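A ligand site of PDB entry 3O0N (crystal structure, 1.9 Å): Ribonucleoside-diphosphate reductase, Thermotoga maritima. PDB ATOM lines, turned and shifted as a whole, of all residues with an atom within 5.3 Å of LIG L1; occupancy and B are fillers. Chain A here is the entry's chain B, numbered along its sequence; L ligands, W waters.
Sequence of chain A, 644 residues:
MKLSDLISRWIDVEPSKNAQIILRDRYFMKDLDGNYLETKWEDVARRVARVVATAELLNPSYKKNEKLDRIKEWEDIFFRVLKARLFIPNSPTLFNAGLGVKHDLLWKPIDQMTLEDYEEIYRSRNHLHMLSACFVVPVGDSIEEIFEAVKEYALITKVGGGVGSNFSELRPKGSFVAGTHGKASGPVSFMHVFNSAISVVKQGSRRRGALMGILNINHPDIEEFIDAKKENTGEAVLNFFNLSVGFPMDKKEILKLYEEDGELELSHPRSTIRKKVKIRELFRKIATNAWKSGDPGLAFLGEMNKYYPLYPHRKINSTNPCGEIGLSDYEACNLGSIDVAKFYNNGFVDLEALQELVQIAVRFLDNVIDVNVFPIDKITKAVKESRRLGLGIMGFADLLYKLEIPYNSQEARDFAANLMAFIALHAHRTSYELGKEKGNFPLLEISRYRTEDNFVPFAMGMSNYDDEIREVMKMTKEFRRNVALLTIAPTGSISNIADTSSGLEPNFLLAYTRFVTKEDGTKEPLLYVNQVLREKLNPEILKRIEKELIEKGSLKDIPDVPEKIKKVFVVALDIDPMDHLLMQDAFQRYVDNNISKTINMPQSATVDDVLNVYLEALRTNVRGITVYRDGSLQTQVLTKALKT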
ATOM      1  N   ILE A  22      -5.423 -20.136 -18.588  1.00  0.00           N
ATOM      2  CA  ILE A  22      -5.362 -21.194 -17.597  1.00  0.00           C
ATOM      3  C   ILE A  22      -6.687 -21.343 -16.871  1.00  0.00           C
ATOM      4  O   ILE A  22      -7.163 -22.455 -16.644  1.00  0.00           O
ATOM      5  CB  ILE A  22      -4.282 -20.901 -16.554  1.00  0.00           C
ATOM      6  CG1 ILE A  22      -2.918 -20.764 -17.237  1.00  0.00           C
ATOM      7  CG2 ILE A  22      -4.271 -21.977 -15.473  1.00  0.00           C
ATOM      8  CD1 ILE A  22      -1.743 -20.646 -16.263  1.00  0.00           C
ATOM      9  N   ARG A  26      -9.092 -24.819 -17.044  1.00  0.00           N
ATOM     10  CA  ARG A  26      -9.208 -25.767 -15.943  1.00  0.00           C
ATOM     11  C   ARG A  26      -9.999 -25.317 -14.715  1.00  0.00           C
ATOM     12  O   ARG A  26     -10.445 -26.146 -13.927  1.00  0.00           O
ATOM     13  CB  ARG A  26      -7.800 -26.213 -15.493  1.00  0.00           C
ATOM     14  CG  ARG A  26      -6.856 -26.488 -16.651  1.00  0.00           C
ATOM     15  CD  ARG A  26      -5.610 -27.267 -16.215  1.00  0.00           C
ATOM     16  NE  ARG A  26      -4.675 -26.471 -15.423  1.00  0.00           N
ATOM     17  CZ  ARG A  26      -3.793 -25.631 -15.935  1.00  0.00           C
ATOM     18  NH1 ARG A  26      -3.722 -25.455 -17.258  1.00  0.00           N
ATOM     19  NH2 ARG A  26      -2.968 -24.949 -15.140  1.00  0.00           N
ATOM     20  N   ALA A 210       2.856 -37.292 -10.055  1.00  0.00           N
ATOM     21  CA  ALA A 210       1.573 -37.247  -9.355  1.00  0.00           C
ATOM     22  C   ALA A 210       1.600 -38.052  -8.061  1.00  0.00           C
ATOM     23  O   ALA A 210       0.717 -37.895  -7.214  1.00  0.00           O
ATOM     24  CB  ALA A 210       0.427 -37.722 -10.275  1.00  0.00           C
ATOM     25  N   ASN A 242       7.267 -39.655  -8.272  1.00  0.00           N
ATOM     26  CA  ASN A 242       8.519 -39.021  -7.859  1.00  0.00           C
ATOM     27  C   ASN A 242       9.093 -39.905  -6.785  1.00  0.00           C
ATOM     28  O   ASN A 242       8.374 -40.372  -5.905  1.00  0.00           O
ATOM     29  CB  ASN A 242       8.306 -37.657  -7.247  1.00  0.00           C
ATOM     30  CG  ASN A 242       7.757 -36.662  -8.215  1.00  0.00           C
ATOM     31  OD1 ASN A 242       8.203 -36.580  -9.359  1.00  0.00           O
ATOM     32  ND2 ASN A 242       6.787 -35.883  -7.753  1.00  0.00           N
ATOM     33  N   SER A 293      19.540 -37.754 -14.052  1.00  0.00           N
ATOM     34  CA  SER A 293      18.095 -37.708 -14.278  1.00  0.00           C
ATOM     35  C   SER A 293      17.298 -36.858 -13.287  1.00  0.00           C
ATOM     36  O   SER A 293      16.102 -36.667 -13.496  1.00  0.00           O
ATOM     37  CB  SER A 293      17.551 -39.119 -14.185  1.00  0.00           C
ATOM     38  OG  SER A 293      17.457 -39.489 -12.820  1.00  0.00           O
ATOM     39  N   GLY A 294      17.925 -36.401 -12.208  1.00  0.00           N
ATOM     40  CA  GLY A 294      17.224 -35.563 -11.240  1.00  0.00           C
ATOM     41  C   GLY A 294      16.463 -36.322 -10.163  1.00  0.00           C
ATOM     42  O   GLY A 294      15.738 -35.723  -9.371  1.00  0.00           O
ATOM     43  N   ASP A 295      16.617 -37.645 -10.158  1.00  0.00           N
ATOM     44  CA  ASP A 295      15.978 -38.512  -9.165  1.00  0.00           C
ATOM     45  C   ASP A 295      16.980 -39.596  -8.727  1.00  0.00           C
ATOM     46  O   ASP A 295      17.916 -39.915  -9.457  1.00  0.00           O
ATOM     47  CB  ASP A 295      14.720 -39.170  -9.746  1.00  0.00           C
ATOM     48  CG  ASP A 295      13.514 -38.217  -9.801  1.00  0.00           C
ATOM     49  OD1 ASP A 295      12.801 -38.075  -8.777  1.00  0.00           O
ATOM     50  OD2 ASP A 295      13.286 -37.607 -10.865  1.00  0.00           O
ATOM     51  N   PRO A 321       3.433 -35.728  -3.029  1.00  0.00           N
ATOM     52  CA  PRO A 321       4.283 -35.874  -4.231  1.00  0.00           C
ATOM     53  C   PRO A 321       5.365 -34.810  -4.409  1.00  0.00           C
ATOM     54  O   PRO A 321       6.446 -35.162  -4.876  1.00  0.00           O
ATOM     55  CB  PRO A 321       3.277 -35.831  -5.391  1.00  0.00           C
ATOM     56  CG  PRO A 321       2.007 -36.411  -4.777  1.00  0.00           C
ATOM     57  CD  PRO A 321       1.991 -35.793  -3.375  1.00  0.00           C
ATOM     58  N   CYS A 322       5.093 -33.545  -4.072  1.00  0.00           N
ATOM     59  CA  CYS A 322       6.084 -32.480  -4.256  1.00  0.00           C
ATOM     60  C   CYS A 322       6.928 -32.194  -3.002  1.00  0.00           C
ATOM     61  O   CYS A 322       7.711 -31.230  -2.963  1.00  0.00           O
ATOM     62  CB  CYS A 322       5.420 -31.198  -4.758  1.00  0.00           C
ATOM     63  SG  CYS A 322       4.533 -31.360  -6.334  1.00  0.00           S
ATOM     64  N   PRO A 490       5.198 -25.644  -4.474  1.00  0.00           N
ATOM     65  CA  PRO A 490       5.664 -25.215  -5.804  1.00  0.00           C
ATOM     66  C   PRO A 490       4.843 -24.021  -6.328  1.00  0.00           C
ATOM     67  O   PRO A 490       5.389 -23.131  -6.994  1.00  0.00           O
ATOM     68  CB  PRO A 490       5.363 -26.450  -6.690  1.00  0.00           C
ATOM     69  CG  PRO A 490       5.249 -27.596  -5.738  1.00  0.00           C
ATOM     70  CD  PRO A 490       4.690 -27.031  -4.455  1.00  0.00           C
ATOM     71  N   GLY A 492       2.948 -23.957  -8.789  1.00  0.00           N
ATOM     72  CA  GLY A 492       3.037 -23.933 -10.237  1.00  0.00           C
ATOM     73  C   GLY A 492       1.861 -23.304 -10.959  1.00  0.00           C
ATOM     74  O   GLY A 492       2.053 -22.443 -11.814  1.00  0.00           O
ATOM     75  N   SER A 493       0.649 -23.702 -10.628  1.00  0.00           N
ATOM     76  CA  SER A 493      -0.516 -23.107 -11.293  1.00  0.00           C
ATOM     77  C   SER A 493      -1.056 -21.822 -10.640  1.00  0.00           C
ATOM     78  O   SER A 493      -1.417 -20.861 -11.330  1.00  0.00           O
ATOM     79  CB  SER A 493      -1.640 -24.134 -11.474  1.00  0.00           C
ATOM     80  OG  SER A 493      -1.419 -24.926 -12.629  1.00  0.00           O
ATOM     81  N   ASN A 496       0.817 -18.614 -11.451  1.00  0.00           N
ATOM     82  CA  ASN A 496       0.437 -18.136 -12.775  1.00  0.00           C
ATOM     83  C   ASN A 496      -0.892 -17.372 -12.797  1.00  0.00           C
ATOM     84  O   ASN A 496      -1.016 -16.332 -13.440  1.00  0.00           O
ATOM     85  CB  ASN A 496       0.389 -19.281 -13.788  1.00  0.00           C
ATOM     86  CG  ASN A 496       1.769 -19.666 -14.289  1.00  0.00           C
ATOM     87  OD1 ASN A 496       2.115 -20.851 -14.357  1.00  0.00           O
ATOM     88  ND2 ASN A 496       2.573 -18.671 -14.631  1.00  0.00           N
ATOM     89  N   SER A 502       7.012 -18.179  -8.577  1.00  0.00           N
ATOM     90  CA  SER A 502       6.520 -19.377  -7.893  1.00  0.00           C
ATOM     91  C   SER A 502       7.191 -19.587  -6.555  1.00  0.00           C
ATOM     92  O   SER A 502       8.426 -19.582  -6.467  1.00  0.00           O
ATOM     93  CB  SER A 502       6.694 -20.637  -8.762  1.00  0.00           C
ATOM     94  OG  SER A 502       6.097 -20.449 -10.035  1.00  0.00           O
ATOM     95  N   GLU A 505      11.017 -19.926  -5.134  1.00  0.00           N
ATOM     96  CA  GLU A 505      11.974 -20.137  -6.228  1.00  0.00           C
ATOM     97  C   GLU A 505      12.352 -18.847  -6.919  1.00  0.00           C
ATOM     98  O   GLU A 505      11.511 -17.971  -7.102  1.00  0.00           O
ATOM     99  CB  GLU A 505      11.393 -21.091  -7.283  1.00  0.00           C
ATOM    100  CG  GLU A 505      11.169 -22.512  -6.812  1.00  0.00           C
ATOM    101  CD  GLU A 505      12.461 -23.303  -6.571  1.00  0.00           C
ATOM    102  OE1 GLU A 505      13.558 -22.785  -6.858  1.00  0.00           O
ATOM    103  OE2 GLU A 505      12.352 -24.466  -6.107  1.00  0.00           O
ATOM    104  N   PHE A 508      12.743 -18.798 -13.187  1.00  0.00           N
ATOM    105  CA  PHE A 508      13.612 -19.672 -13.967  1.00  0.00           C
ATOM    106  C   PHE A 508      14.126 -18.941 -15.201  1.00  0.00           C
ATOM    107  O   PHE A 508      15.261 -19.145 -15.625  1.00  0.00           O
ATOM    108  CB  PHE A 508      12.935 -20.987 -14.368  1.00  0.00           C
ATOM    109  CG  PHE A 508      13.906 -21.993 -14.914  1.00  0.00           C
ATOM    110  CD1 PHE A 508      14.085 -22.125 -16.276  1.00  0.00           C
ATOM    111  CD2 PHE A 508      14.692 -22.746 -14.063  1.00  0.00           C
ATOM    112  CE1 PHE A 508      15.010 -23.013 -16.777  1.00  0.00           C
ATOM    113  CE2 PHE A 508      15.610 -23.642 -14.556  1.00  0.00           C
ATOM    114  CZ  PHE A 508      15.773 -23.778 -15.912  1.00  0.00           C
ATOM    115  N   ARG A 514       5.510 -20.770 -22.996  1.00  0.00           N
ATOM    116  CA  ARG A 514       5.027 -22.115 -22.658  1.00  0.00           C
ATOM    117  C   ARG A 514       3.863 -22.526 -23.565  1.00  0.00           C
ATOM    118  O   ARG A 514       3.352 -21.717 -24.336  1.00  0.00           O
ATOM    119  CB  ARG A 514       4.594 -22.194 -21.186  1.00  0.00           C
ATOM    120  CG  ARG A 514       5.683 -21.845 -20.184  1.00  0.00           C
ATOM    121  CD  ARG A 514       5.181 -22.032 -18.749  1.00  0.00           C
ATOM    122  NE  ARG A 514       5.982 -21.290 -17.777  1.00  0.00           N
ATOM    123  CZ  ARG A 514       5.769 -21.294 -16.461  1.00  0.00           C
ATOM    124  NH1 ARG A 514       6.559 -20.584 -15.658  1.00  0.00           N
ATOM    125  NH2 ARG A 514       4.775 -22.011 -15.947  1.00  0.00           N
ATOM    126  N   THR A 598      13.924 -26.699  -5.755  1.00  0.00           N
ATOM    127  CA  THR A 598      14.834 -27.416  -6.623  1.00  0.00           C
ATOM    128  C   THR A 598      16.225 -26.834  -6.470  1.00  0.00           C
ATOM    129  O   THR A 598      16.402 -25.628  -6.601  1.00  0.00           O
ATOM    130  CB  THR A 598      14.421 -27.319  -8.109  1.00  0.00           C
ATOM    131  OG1 THR A 598      13.192 -28.022  -8.303  1.00  0.00           O
ATOM    132  CG2 THR A 598      15.516 -27.946  -8.999  1.00  0.00           C
ATOM    133  N   ASN A 600      18.917 -26.186  -8.426  1.00  0.00           N
ATOM    134  CA  ASN A 600      19.434 -26.082  -9.790  1.00  0.00           C
ATOM    135  C   ASN A 600      20.963 -26.072  -9.844  1.00  0.00           C
ATOM    136  O   ASN A 600      21.614 -25.332  -9.105  1.00  0.00           O
ATOM    137  CB  ASN A 600      18.907 -24.807 -10.439  1.00  0.00           C
ATOM    138  CG  ASN A 600      17.390 -24.766 -10.487  1.00  0.00           C
ATOM    139  OD1 ASN A 600      16.759 -24.140  -9.647  1.00  0.00           O
ATOM    140  ND2 ASN A 600      16.815 -25.476 -11.446  1.00  0.00           N
ATOM    141  N   THR A 626      16.174 -31.782  -3.433  1.00  0.00           N
ATOM    142  CA  THR A 626      15.922 -32.158  -4.810  1.00  0.00           C
ATOM    143  C   THR A 626      16.977 -31.398  -5.590  1.00  0.00           C
ATOM    144  O   THR A 626      17.119 -30.185  -5.419  1.00  0.00           O
ATOM    145  CB  THR A 626      14.526 -31.651  -5.270  1.00  0.00           C
ATOM    146  OG1 THR A 626      13.479 -32.329  -4.564  1.00  0.00           O
ATOM    147  CG2 THR A 626      14.340 -31.870  -6.738  1.00  0.00           C
ATOM    148  N   VAL A 627      17.726 -32.093  -6.435  1.00  0.00           N
ATOM    149  CA  VAL A 627      18.615 -31.392  -7.346  1.00  0.00           C
ATOM    150  C   VAL A 627      18.216 -31.643  -8.792  1.00  0.00           C
ATOM    151  O   VAL A 627      17.663 -32.679  -9.115  1.00  0.00           O
ATOM    152  CB  VAL A 627      20.101 -31.804  -7.155  1.00  0.00           C
ATOM    153  CG1 VAL A 627      20.524 -31.611  -5.699  1.00  0.00           C
ATOM    154  CG2 VAL A 627      20.300 -33.236  -7.581  1.00  0.00           C
ATOM    155  N   TYR A 628      18.499 -30.680  -9.655  1.00  0.00           N
ATOM    156  CA  TYR A 628      18.437 -30.909 -11.086  1.00  0.00           C
ATOM    157  C   TYR A 628      19.587 -30.246 -11.812  1.00  0.00           C
ATOM    158  O   TYR A 628      19.776 -29.025 -11.732  1.00  0.00           O
ATOM    159  CB  TYR A 628      17.112 -30.443 -11.689  1.00  0.00           C
ATOM    160  CG  TYR A 628      17.055 -30.772 -13.156  1.00  0.00           C
ATOM    161  CD1 TYR A 628      16.912 -32.091 -13.574  1.00  0.00           C
ATOM    162  CD2 TYR A 628      17.197 -29.784 -14.125  1.00  0.00           C
ATOM    163  CE1 TYR A 628      16.879 -32.412 -14.919  1.00  0.00           C
ATOM    164  CE2 TYR A 628      17.161 -30.091 -15.471  1.00  0.00           C
ATOM    165  CZ  TYR A 628      17.004 -31.418 -15.861  1.00  0.00           C
ATOM    166  OH  TYR A 628      16.977 -31.742 -17.194  1.00  0.00           O
ATOM    167  N   ASP A 630      21.224 -28.867 -15.065  1.00  0.00           N
ATOM    168  CA  ASP A 630      20.833 -28.329 -16.364  1.00  0.00           C
ATOM    169  C   ASP A 630      21.408 -29.176 -17.505  1.00  0.00           C
ATOM    170  O   ASP A 630      22.617 -29.277 -17.661  1.00  0.00           O
ATOM    171  CB  ASP A 630      21.330 -26.901 -16.502  1.00  0.00           C
ATOM    172  CG  ASP A 630      20.899 -26.242 -17.807  1.00  0.00           C
ATOM    173  OD1 ASP A 630      21.788 -25.699 -18.503  1.00  0.00           O
ATOM    174  OD2 ASP A 630      19.683 -26.233 -18.109  1.00  0.00           O
ATOM    175  N   LEU A 633      18.132 -34.231 -18.460  1.00  0.00           N
ATOM    176  CA  LEU A 633      17.099 -34.852 -19.278  1.00  0.00           C
ATOM    177  C   LEU A 633      17.025 -34.206 -20.653  1.00  0.00           C
ATOM    178  O   LEU A 633      17.610 -34.706 -21.617  1.00  0.00           O
ATOM    179  CB  LEU A 633      15.743 -34.760 -18.570  1.00  0.00           C
ATOM    180  CG  LEU A 633      15.674 -35.372 -17.166  1.00  0.00           C
ATOM    181  CD1 LEU A 633      14.245 -35.380 -16.654  1.00  0.00           C
ATOM    182  CD2 LEU A 633      16.243 -36.777 -17.159  1.00  0.00           C
HETATM  183 CO1  LIG L   1       9.318 -30.103 -12.222  1.00  0.00          CO
HETATM  184  N1  LIG L   1      10.511 -28.928 -13.113  1.00  0.00           N
HETATM  185  N2  LIG L   1      10.585 -31.534 -12.379  1.00  0.00           N
HETATM  186  N3  LIG L   1       7.932 -31.111 -11.374  1.00  0.00           N
HETATM  187  N4  LIG L   1       8.248 -28.577 -12.082  1.00  0.00           N
HETATM  188  C1  LIG L   1      10.067 -27.552 -13.521  1.00  0.00           C
HETATM  189  C2  LIG L   1       9.602 -27.498 -14.989  1.00  0.00           C
HETATM  190  C3  LIG L   1      11.389 -26.713 -13.242  1.00  0.00           C
HETATM  191  C4  LIG L   1      11.495 -25.362 -13.975  1.00  0.00           C
HETATM  192  C5  LIG L   1      11.615 -26.523 -11.688  1.00  0.00           C
HETATM  193  C6  LIG L   1      12.870 -25.755 -11.280  1.00  0.00           C
HETATM  194  O1  LIG L   1      13.923 -25.874 -11.900  1.00  0.00           O
HETATM  195  N5  LIG L   1      12.769 -24.945 -10.215  1.00  0.00           N
HETATM  196  C7  LIG L   1      12.463 -27.745 -13.714  1.00  0.00           C
HETATM  197  C8  LIG L   1      12.899 -27.743 -15.213  1.00  0.00           C
HETATM  198  C9  LIG L   1      14.345 -27.247 -15.448  1.00  0.00           C
HETATM  199  C10 LIG L   1      14.631 -27.228 -16.930  1.00  0.00           C
HETATM  200  O2  LIG L   1      13.796 -27.668 -17.737  1.00  0.00           O
HETATM  201  N6  LIG L   1      15.800 -26.714 -17.300  1.00  0.00           N
HETATM  202  C11 LIG L   1      11.791 -29.059 -13.319  1.00  0.00           C
HETATM  203  C12 LIG L   1      12.537 -30.278 -13.151  1.00  0.00           C
HETATM  204  C13 LIG L   1      14.009 -30.198 -13.497  1.00  0.00           C
HETATM  205  C14 LIG L   1      11.944 -31.434 -12.707  1.00  0.00           C
HETATM  206  C15 LIG L   1      12.670 -32.772 -12.488  1.00  0.00           C
HETATM  207  C16 LIG L   1      13.429 -33.390 -13.677  1.00  0.00           C
HETATM  208  C17 LIG L   1      13.676 -32.510 -11.340  1.00  0.00           C
HETATM  209  O3  LIG L   1      13.087 -34.332  -9.845  1.00  0.00           O
HETATM  210  N7  LIG L   1      14.800 -32.950  -9.335  1.00  0.00           N
HETATM  211  C18 LIG L   1      11.501 -33.708 -12.049  1.00  0.00           C
HETATM  212  C19 LIG L   1      11.229 -34.841 -13.077  1.00  0.00           C
HETATM  213  C20 LIG L   1      10.007 -34.671 -14.014  1.00  0.00           C
HETATM  214  C21 LIG L   1      10.476 -33.990 -15.301  1.00  0.00           C
HETATM  215  O4  LIG L   1      10.283 -34.505 -16.393  1.00  0.00           O
HETATM  216  N8  LIG L   1      11.079 -32.814 -15.157  1.00  0.00           N
HETATM  217  C22 LIG L   1      10.331 -32.771 -11.915  1.00  0.00           C
HETATM  218  C23 LIG L   1       8.018 -32.405 -11.108  1.00  0.00           C
HETATM  219  C24 LIG L   1       6.734 -32.957 -10.478  1.00  0.00           C
HETATM  220  C25 LIG L   1       6.939 -33.426  -9.071  1.00  0.00           C
HETATM  221  C26 LIG L   1       6.271 -34.171 -11.341  1.00  0.00           C
HETATM  222  C27 LIG L   1       5.750 -31.794 -10.694  1.00  0.00           C
HETATM  223  C28 LIG L   1       4.573 -31.742 -11.781  1.00  0.00           C
HETATM  224  C29 LIG L   1       3.368 -32.421 -11.279  1.00  0.00           C
HETATM  225  C30 LIG L   1       2.588 -31.494 -10.359  1.00  0.00           C
HETATM  226  O5  LIG L   1       2.192 -30.401 -10.762  1.00  0.00           O
HETATM  227  N9  LIG L   1       2.373 -31.929  -9.089  1.00  0.00           N
HETATM  228  C31 LIG L   1       6.695 -30.642 -10.959  1.00  0.00           C
HETATM  229  C32 LIG L   1       6.363 -29.338 -10.808  1.00  0.00           C
HETATM  230  C33 LIG L   1       5.086 -28.917  -9.986  1.00  0.00           C
HETATM  231  C34 LIG L   1       7.181 -28.289 -11.399  1.00  0.00           C
HETATM  232  C35 LIG L   1       6.922 -26.778 -11.319  1.00  0.00           C
HETATM  233  C36 LIG L   1       7.329 -26.292  -9.910  1.00  0.00           C
HETATM  234  C37 LIG L   1       5.457 -26.363 -11.639  1.00  0.00           C
HETATM  235  C38 LIG L   1       5.168 -26.093 -13.115  1.00  0.00           C
HETATM  236  C39 LIG L   1       3.664 -26.015 -13.360  1.00  0.00           C
HETATM  237  O6  LIG L   1       2.852 -26.649 -12.690  1.00  0.00           O
HETATM  238  N10 LIG L   1       3.332 -25.190 -14.371  1.00  0.00           N
HETATM  239  C40 LIG L   1       7.883 -26.174 -12.392  1.00  0.00           C
HETATM  240  C41 LIG L   1       8.570 -24.864 -11.999  1.00  0.00           C
HETATM  241  C42 LIG L   1       7.598 -23.713 -12.159  1.00  0.00           C
HETATM  242  O7  LIG L   1       7.066 -23.186 -11.170  1.00  0.00           O
HETATM  243  N11 LIG L   1       7.363 -23.328 -13.394  1.00  0.00           N
HETATM  244  C43 LIG L   1       8.796 -27.359 -12.687  1.00  0.00           C
HETATM  245  C44 LIG L   1       1.957 -24.917 -14.731  1.00  0.00           C
HETATM  246  C45 LIG L   1       0.016 -25.205 -16.315  1.00  0.00           C
HETATM  247  O8  LIG L   1       2.259 -25.516 -17.103  1.00  0.00           O
HETATM  248  O9  LIG L   1       4.086 -26.389 -18.557  1.00  0.00           O
HETATM  249  O10 LIG L   1       1.777 -27.391 -18.707  1.00  0.00           O
HETATM  250  P1  LIG L   1       2.830 -26.783 -17.863  1.00  0.00           P
HETATM  251  O11 LIG L   1       3.205 -27.743 -16.625  1.00  0.00           O
HETATM  252  C46 LIG L   1       3.576 -29.104 -16.845  1.00  0.00           C
HETATM  253  C47 LIG L   1       5.058 -29.275 -17.199  1.00  0.00           C
HETATM  254  O12 LIG L   1       5.830 -28.180 -16.761  1.00  0.00           O
HETATM  255  C48 LIG L   1       5.425 -30.555 -16.390  1.00  0.00           C
HETATM  256  O13 LIG L   1       4.481 -30.803 -15.367  1.00  0.00           O
HETATM  257  C49 LIG L   1       2.010 -30.519 -15.450  1.00  0.00           C
HETATM  258  O14 LIG L   1       1.884 -31.105 -14.232  1.00  0.00           O
HETATM  259  N12 LIG L   1       6.772 -30.569 -15.807  1.00  0.00           N
HETATM  260  C50 LIG L   1       7.946 -30.416 -16.496  1.00  0.00           C
HETATM  261  C51 LIG L   1       7.105 -30.778 -14.477  1.00  0.00           C
HETATM  262  N13 LIG L   1       8.420 -30.738 -14.252  1.00  0.00           N
HETATM  263  C52 LIG L   1       8.964 -30.523 -15.518  1.00  0.00           C
HETATM  264  C53 LIG L   1      10.308 -30.397 -15.904  1.00  0.00           C
HETATM  265  C54 LIG L   1      10.609 -30.177 -17.243  1.00  0.00           C
HETATM  266  C55 LIG L   1      11.985 -30.043 -17.641  1.00  0.00           C
HETATM  267  C56 LIG L   1       9.537 -30.061 -18.259  1.00  0.00           C
HETATM  268  C57 LIG L   1       9.865 -29.809 -19.706  1.00  0.00           C
HETATM  269  C58 LIG L   1       8.208 -30.186 -17.848  1.00  0.00           C
HETATM  270  N1  LG2 L   2      10.822 -35.056  -3.662  1.00  0.00           N
HETATM  271  C1  LG2 L   2      10.119 -33.868  -3.430  1.00  0.00           C
HETATM  272  N2  LG2 L   2       9.765 -33.100  -4.539  1.00  0.00           N
HETATM  273  C2  LG2 L   2      10.108 -33.508  -5.767  1.00  0.00           C
HETATM  274  N3  LG2 L   2       9.881 -32.941  -6.945  1.00  0.00           N
HETATM  275  C3  LG2 L   2      10.414 -33.722  -7.881  1.00  0.00           C
HETATM  276  N4  LG2 L   2      10.969 -34.770  -7.276  1.00  0.00           N
HETATM  277  C4  LG2 L   2      10.780 -34.640  -5.959  1.00  0.00           C
HETATM  278  C5  LG2 L   2      11.126 -35.396  -4.916  1.00  0.00           C
HETATM  279  N5  LG2 L   2      11.798 -36.521  -5.170  1.00  0.00           N
HETATM  280  C6  LG2 L   2       9.151 -31.661  -7.027  1.00  0.00           C
HETATM  281  C7  LG2 L   2       9.949 -30.575  -6.319  1.00  0.00           C
HETATM  282  C8  LG2 L   2       9.680 -29.320  -7.140  1.00  0.00           C
HETATM  283  C9  LG2 L   2       8.951 -29.809  -8.394  1.00  0.00           C
HETATM  284  C10 LG2 L   2       9.729 -29.291  -9.592  1.00  0.00           C
HETATM  285  O1  LG2 L   2       9.041 -31.234  -8.393  1.00  0.00           O
HETATM  286  O2  LG2 L   2       9.469 -30.416  -4.965  1.00  0.00           O
HETATM  287  O3  LG2 L   2       8.826 -28.403  -6.410  1.00  0.00           O
HETATM  288  O   HOH W   1      14.760 -22.832  -9.139  1.00  0.00           O
HETATM  289  O   HOH W   2      17.987 -26.599 -16.075  1.00  0.00           O
HETATM  290  O   HOH W   3      10.749 -25.537  -8.644  1.00  0.00           O
HETATM  291  O   HOH W   4      12.827 -30.937  -9.026  1.00  0.00           O
HETATM  292  O   HOH W   5      13.897 -35.280  -6.681  1.00  0.00           O
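A nitrogen (N7) of LIG L1 sits at hydrogen-bond distance from the backbone carbonyl oxygen (O) of Val 627, 2.9 Å away. O of Gly 294 lies within hydrogen-bond range of N7 of LIG L1. ND2 of Asn 600 is in hydrogen-bond range of O1 of LIG L1 (3.0 Å). The side-chain hydroxyl of Ser 502 sits at hydrogen-bond distance from an oxygen (O7) of LIG L1 (3.1 Å). SG of Cys 322 lies within hydrogen-bond range of N9 of LIG L1. An oxygen (O2) of LG2 L2 is in hydrogen-bond range of the backbone carbonyl oxygen of Cys 322, at 2.8 Å.
Water W2 bridges N6 of LIG L1 and OD2 of Asp 630. Water W3 lies within hydrogen-bond range of N5 of LIG L1 and OE2 of Glu 505. Water W4 bridges N7 of LIG L1 (2.8 Å) and OG1 of Thr 598 (3.0 Å). Water W1 lies within hydrogen-bond range of the side-chain amide oxygen of Asn 600, the side-chain carboxylate of Glu 505 and a nitrogen (N5) of LIG L1. Water W5 lies within hydrogen-bond range of N5 of LG2 L2 (2.9 Å), O of Gly 294 (3.3 Å) and O3 of LIG L1 (3.4 Å).
An oxygen (O3) of LIG L1 sits close to the side-chain carboxylate (OD2) of Asp 295 (3.4 Å). NH2 of Arg 26 touches C45 of LIG L1, at 3.2 Å. ND2 of Asn 242 touches C25 of LIG L1, 2.8 Å away. Pro 490 touches LIG L1. Gly 492 touches LIG L1. Ser 493 touches LIG L1 (OG to C45, 3.97 Å). CZ of Phe 508 touches N6 of LIG L1, at 3.2 Å. Arg 514 touches LIG L1. CB of Thr 598 touches N5 of LIG L1, 3.6 Å away. Thr 626 touches LIG L1. CG of Tyr 628 touches C13 of LIG L1, 3.1 Å away. Asp 630 touches LIG L1. CD1 of Leu 633 touches C16 of LIG L1 (3.7 Å). 18 residues have an atom within 4 Å of LIG L1: Arg 26, Asn 242, Gly 294, Asp 295, Cys 322, Pro 490, Gly 492, Ser 493, Ser 502, Phe 508, Arg 514, Thr 598, Asn 600, Thr 626, Val 627, Tyr 628, Asp 630 and Leu 633.
O of Pro 321 sits at hydrogen-bond distance from ND2 of Asn 242 (3.0 Å). OD1 of Asn 600 lies close to O of Thr 598, 3.4 Å away. The backbone NH of Leu 633 is in hydrogen-bond range of the side-chain hydroxyl of Tyr 628. The guanidinium group (NH2) of Arg 26 sits at hydrogen-bond distance from the side-chain hydroxyl (OG) of Ser 493, 3.0 Å away. N of Asp 295 sits close to OG of Ser 293. OE2 of Glu 505 lies within hydrogen-bond range of N of Thr 598, at 2.8 Å. The guanidinium group (NH2) of Arg 514 is in hydrogen-bond range of the side-chain amide oxygen (OD1) of Asn 496, at 3.3 Å. The backbone carbonyl oxygen of Gly 492 lies close to the side-chain amide oxygen of Asn 496 (3.0 Å).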
